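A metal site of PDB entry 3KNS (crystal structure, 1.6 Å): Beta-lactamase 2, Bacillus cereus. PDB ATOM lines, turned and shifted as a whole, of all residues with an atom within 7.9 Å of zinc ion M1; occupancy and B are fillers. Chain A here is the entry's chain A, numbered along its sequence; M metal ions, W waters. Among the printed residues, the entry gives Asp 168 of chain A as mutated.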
ATOM      1  N   TRP A  59      -5.049 -21.095 -18.028  1.00  0.00           N
ATOM      2  CA  TRP A  59      -4.377 -22.022 -18.906  1.00  0.00           C
ATOM      3  C   TRP A  59      -4.900 -22.066 -20.299  1.00  0.00           C
ATOM      4  O   TRP A  59      -4.180 -22.391 -21.251  1.00  0.00           O
ATOM      5  CB  TRP A  59      -4.526 -23.413 -18.328  1.00  0.00           C
ATOM      6  CG  TRP A  59      -3.918 -23.641 -17.002  1.00  0.00           C
ATOM      7  CD1 TRP A  59      -4.542 -23.646 -15.811  1.00  0.00           C
ATOM      8  CD2 TRP A  59      -2.555 -23.961 -16.754  1.00  0.00           C
ATOM      9  NE1 TRP A  59      -3.670 -23.964 -14.811  1.00  0.00           N
ATOM     10  CE2 TRP A  59      -2.425 -24.125 -15.360  1.00  0.00           C
ATOM     11  CE3 TRP A  59      -1.454 -24.112 -17.569  1.00  0.00           C
ATOM     12  CZ2 TRP A  59      -1.252 -24.478 -14.775  1.00  0.00           C
ATOM     13  CZ3 TRP A  59      -0.243 -24.436 -16.953  1.00  0.00           C
ATOM     14  CH2 TRP A  59      -0.174 -24.638 -15.588  1.00  0.00           C
ATOM     15  N   HIS A  86       3.591 -13.234 -18.393  1.00  0.00           N
ATOM     16  CA  HIS A  86       4.483 -13.703 -19.431  1.00  0.00           C
ATOM     17  C   HIS A  86       3.677 -14.432 -20.447  1.00  0.00           C
ATOM     18  O   HIS A  86       2.487 -14.674 -20.245  1.00  0.00           O
ATOM     19  CB  HIS A  86       5.733 -14.477 -18.927  1.00  0.00           C
ATOM     20  CG  HIS A  86       5.490 -15.861 -18.443  1.00  0.00           C
ATOM     21  ND1 HIS A  86       5.047 -16.138 -17.170  1.00  0.00           N
ATOM     22  CD2 HIS A  86       5.703 -17.041 -19.048  1.00  0.00           C
ATOM     23  CE1 HIS A  86       4.973 -17.451 -17.036  1.00  0.00           C
ATOM     24  NE2 HIS A  86       5.335 -18.018 -18.175  1.00  0.00           N
ATOM     25  N   ALA A  87       4.314 -14.780 -21.559  1.00  0.00           N
ATOM     26  CA  ALA A  87       3.599 -15.303 -22.719  1.00  0.00           C
ATOM     27  C   ALA A  87       3.530 -16.821 -22.758  1.00  0.00           C
ATOM     28  O   ALA A  87       3.631 -17.422 -23.857  1.00  0.00           O
ATOM     29  CB  ALA A  87       4.182 -14.756 -24.018  1.00  0.00           C
ATOM     30  N   HIS A  88       3.197 -17.449 -21.644  1.00  0.00           N
ATOM     31  CA  HIS A  88       2.890 -18.874 -21.632  1.00  0.00           C
ATOM     32  C   HIS A  88       1.434 -19.097 -21.209  1.00  0.00           C
ATOM     33  O   HIS A  88       0.796 -18.245 -20.588  1.00  0.00           O
ATOM     34  CB  HIS A  88       3.772 -19.589 -20.596  1.00  0.00           C
ATOM     35  CG  HIS A  88       5.199 -19.790 -21.014  1.00  0.00           C
ATOM     36  ND1 HIS A  88       6.182 -20.112 -20.088  1.00  0.00           N
ATOM     37  CD2 HIS A  88       5.783 -19.770 -22.225  1.00  0.00           C
ATOM     38  CE1 HIS A  88       7.320 -20.293 -20.752  1.00  0.00           C
ATOM     39  NE2 HIS A  88       7.114 -20.064 -22.038  1.00  0.00           N
ATOM     40  N   ALA A  89       0.961 -20.342 -21.419  1.00  0.00           N
ATOM     41  CA  ALA A  89      -0.453 -20.653 -21.332  1.00  0.00           C
ATOM     42  C   ALA A  89      -1.075 -20.333 -19.992  1.00  0.00           C
ATOM     43  O   ALA A  89      -2.208 -19.859 -19.934  1.00  0.00           O
ATOM     44  CB  ALA A  89      -0.667 -22.145 -21.617  1.00  0.00           C
ATOM     45  N   ASP A  90      -0.349 -20.595 -18.917  1.00  0.00           N
ATOM     46  CA  ASP A  90      -0.941 -20.311 -17.626  1.00  0.00           C
ATOM     47  C   ASP A  90      -1.277 -18.876 -17.375  1.00  0.00           C
ATOM     48  O   ASP A  90      -2.118 -18.566 -16.521  1.00  0.00           O
ATOM     49  CB  ASP A  90      -0.163 -20.881 -16.422  1.00  0.00           C
ATOM     50  CG  ASP A  90       1.314 -20.635 -16.441  1.00  0.00           C
ATOM     51  OD1 ASP A  90       1.879 -20.015 -17.342  1.00  0.00           O
ATOM     52  OD2 ASP A  90       1.898 -21.085 -15.452  1.00  0.00           O
ATOM     53  N   ARG A  91      -0.613 -17.993 -18.110  1.00  0.00           N
ATOM     54  CA  ARG A  91      -0.804 -16.591 -17.997  1.00  0.00           C
ATOM     55  C   ARG A  91      -1.660 -15.995 -19.082  1.00  0.00           C
ATOM     56  O   ARG A  91      -2.547 -15.182 -18.800  1.00  0.00           O
ATOM     57  CB  ARG A  91       0.554 -15.920 -18.032  1.00  0.00           C
ATOM     58  CG  ARG A  91       1.536 -16.591 -17.089  1.00  0.00           C
ATOM     59  CD  ARG A  91       1.103 -16.539 -15.649  1.00  0.00           C
ATOM     60  NE  ARG A  91       1.540 -17.676 -14.892  1.00  0.00           N
ATOM     61  CZ  ARG A  91       1.095 -17.933 -13.658  1.00  0.00           C
ATOM     62  NH1 ARG A  91       0.230 -17.112 -13.093  1.00  0.00           N
ATOM     63  NH2 ARG A  91       1.529 -18.972 -12.995  1.00  0.00           N
ATOM     64  N   HIS A 149      12.377 -16.968 -15.487  1.00  0.00           N
ATOM     65  CA  HIS A 149      11.578 -18.064 -15.972  1.00  0.00           C
ATOM     66  C   HIS A 149      11.443 -18.000 -17.496  1.00  0.00           C
ATOM     67  O   HIS A 149      11.529 -19.004 -18.227  1.00  0.00           O
ATOM     68  CB  HIS A 149      10.221 -18.061 -15.293  1.00  0.00           C
ATOM     69  CG  HIS A 149       9.249 -18.951 -15.948  1.00  0.00           C
ATOM     70  ND1 HIS A 149       9.312 -20.329 -15.882  1.00  0.00           N
ATOM     71  CD2 HIS A 149       8.155 -18.656 -16.689  1.00  0.00           C
ATOM     72  CE1 HIS A 149       8.325 -20.826 -16.581  1.00  0.00           C
ATOM     73  NE2 HIS A 149       7.614 -19.836 -17.079  1.00  0.00           N
ATOM     74  N   THR A 150      11.192 -16.784 -17.998  1.00  0.00           N
ATOM     75  CA  THR A 150      11.238 -16.459 -19.395  1.00  0.00           C
ATOM     76  C   THR A 150      11.978 -15.160 -19.586  1.00  0.00           C
ATOM     77  O   THR A 150      12.279 -14.442 -18.616  1.00  0.00           O
ATOM     78  CB  THR A 150       9.867 -16.302 -19.992  1.00  0.00           C
ATOM     79  OG1 THR A 150       9.137 -15.358 -19.205  1.00  0.00           O
ATOM     80  CG2 THR A 150       9.158 -17.648 -19.995  1.00  0.00           C
ATOM     81  N   ASP A 152      10.672 -12.487 -20.656  1.00  0.00           N
ATOM     82  CA  ASP A 152       9.747 -11.377 -20.541  1.00  0.00           C
ATOM     83  C   ASP A 152       9.007 -11.269 -19.224  1.00  0.00           C
ATOM     84  O   ASP A 152       8.325 -10.276 -18.985  1.00  0.00           O
ATOM     85  CB  ASP A 152       8.676 -11.493 -21.623  1.00  0.00           C
ATOM     86  CG  ASP A 152       7.833 -12.739 -21.513  1.00  0.00           C
ATOM     87  OD1 ASP A 152       8.400 -13.823 -21.320  1.00  0.00           O
ATOM     88  OD2 ASP A 152       6.591 -12.655 -21.626  1.00  0.00           O
ATOM     89  N   ASN A 153       9.177 -12.250 -18.350  1.00  0.00           N
ATOM     90  CA  ASN A 153       8.404 -12.270 -17.119  1.00  0.00           C
ATOM     91  C   ASN A 153       8.409 -10.967 -16.354  1.00  0.00           C
ATOM     92  O   ASN A 153       9.465 -10.355 -16.152  1.00  0.00           O
ATOM     93  CB  ASN A 153       8.790 -13.433 -16.240  1.00  0.00           C
ATOM     94  CG  ASN A 153      10.302 -13.607 -15.977  1.00  0.00           C
ATOM     95  OD1 ASN A 153      10.701 -14.748 -15.747  1.00  0.00           O
ATOM     96  ND2 ASN A 153      11.096 -12.540 -15.959  1.00  0.00           N
ATOM     97  N   GLY A 167       4.217 -14.453 -10.387  1.00  0.00           N
ATOM     98  CA  GLY A 167       4.152 -15.370 -11.480  1.00  0.00           C
ATOM     99  C   GLY A 167       5.212 -16.446 -11.395  1.00  0.00           C
ATOM    100  O   GLY A 167       5.645 -16.806 -10.327  1.00  0.00           O
ATOM    101  N   ASP A 168       5.587 -17.022 -12.526  1.00  0.00           N
ATOM    102  CA  ASP A 168       6.429 -18.185 -12.509  1.00  0.00           C
ATOM    103  C   ASP A 168       7.869 -17.815 -12.169  1.00  0.00           C
ATOM    104  O   ASP A 168       8.645 -18.696 -11.868  1.00  0.00           O
ATOM    105  CB  ASP A 168       6.441 -18.912 -13.873  1.00  0.00           C
ATOM    106  CG  ASP A 168       5.180 -19.683 -14.141  1.00  0.00           C
ATOM    107  OD1 ASP A 168       4.141 -19.043 -14.332  1.00  0.00           O
ATOM    108  OD2 ASP A 168       5.272 -20.907 -14.188  1.00  0.00           O
ATOM    109  N   LEU A 169       8.170 -16.541 -12.092  1.00  0.00           N
ATOM    110  CA  LEU A 169       9.465 -16.086 -11.582  1.00  0.00           C
ATOM    111  C   LEU A 169       9.680 -16.488 -10.138  1.00  0.00           C
ATOM    112  O   LEU A 169      10.818 -16.625  -9.711  1.00  0.00           O
ATOM    113  CB  LEU A 169       9.546 -14.560 -11.698  1.00  0.00           C
ATOM    114  CG  LEU A 169      10.909 -13.933 -11.450  1.00  0.00           C
ATOM    115  CD1 LEU A 169      11.894 -14.197 -12.600  1.00  0.00           C
ATOM    116  CD2 LEU A 169      10.722 -12.450 -11.202  1.00  0.00           C
ATOM    117  N   LYS A 171       8.831 -19.026  -6.961  1.00  0.00           N
ATOM    118  CA  LYS A 171       8.416 -20.316  -6.526  1.00  0.00           C
ATOM    119  C   LYS A 171       7.860 -20.330  -5.147  1.00  0.00           C
ATOM    120  O   LYS A 171       8.258 -19.538  -4.311  1.00  0.00           O
ATOM    121  CB  LYS A 171       9.591 -21.277  -6.571  1.00  0.00           C
ATOM    122  CG  LYS A 171      10.234 -21.379  -7.913  1.00  0.00           C
ATOM    123  CD  LYS A 171       9.266 -21.483  -9.014  1.00  0.00           C
ATOM    124  CE  LYS A 171       9.930 -21.544 -10.319  1.00  0.00           C
ATOM    125  NZ  LYS A 171       8.918 -21.602 -11.412  1.00  0.00           N
ATOM    126  N   ASN A 180      10.200 -25.871 -16.171  1.00  0.00           N
ATOM    127  CA  ASN A 180      10.762 -25.887 -17.475  1.00  0.00           C
ATOM    128  C   ASN A 180      11.727 -24.733 -17.676  1.00  0.00           C
ATOM    129  O   ASN A 180      11.348 -23.577 -17.532  1.00  0.00           O
ATOM    130  CB  ASN A 180       9.628 -25.806 -18.492  1.00  0.00           C
ATOM    131  CG  ASN A 180      10.088 -25.949 -19.885  1.00  0.00           C
ATOM    132  OD1 ASN A 180      11.090 -25.383 -20.282  1.00  0.00           O
ATOM    133  ND2 ASN A 180       9.305 -26.671 -20.697  1.00  0.00           N
ATOM    134  N   HIS A 210       2.538 -20.528  -8.942  1.00  0.00           N
ATOM    135  CA  HIS A 210       1.922 -21.772  -8.585  1.00  0.00           C
ATOM    136  C   HIS A 210       2.219 -22.053  -7.145  1.00  0.00           C
ATOM    137  O   HIS A 210       3.338 -21.880  -6.692  1.00  0.00           O
ATOM    138  CB  HIS A 210       2.571 -22.889  -9.400  1.00  0.00           C
ATOM    139  CG  HIS A 210       2.507 -22.664 -10.865  1.00  0.00           C
ATOM    140  ND1 HIS A 210       1.408 -23.018 -11.620  1.00  0.00           N
ATOM    141  CD2 HIS A 210       3.392 -22.091 -11.721  1.00  0.00           C
ATOM    142  CE1 HIS A 210       1.627 -22.677 -12.874  1.00  0.00           C
ATOM    143  NE2 HIS A 210       2.817 -22.110 -12.960  1.00  0.00           N
HETATM  144 ZN    ZN M   1       5.989 -20.022 -18.202  1.00  0.00          ZN
HETATM  145 ZN    ZN M   2       3.573 -21.621 -14.733  1.00  0.00          ZN
HETATM  146  O   HOH W   1       6.432 -22.330 -18.331  1.00  0.00           O
HETATM  147  O   HOH W   2       4.324 -20.852 -17.412  1.00  0.00           O
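N of His 149 sits at hydrogen-bond distance from OD1 of Asn 153 (2.8 Å).
Zinc ion M1 is bound by a ring nitrogen (ND1) of His 88 (1.9 Å), a ring nitrogen (NE2) of His 149 (2.0 Å), water W2 (2.0 Å), a ring nitrogen (NE2) of His 86 (2.1 Å) and water W1 (2.4 Å).
Of the 17 residues printed, 3 come within 4 Å of zinc ion M1.
The nearest printed residue that does not touch zinc ion M1 is Asp 168 (4.2 Å).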
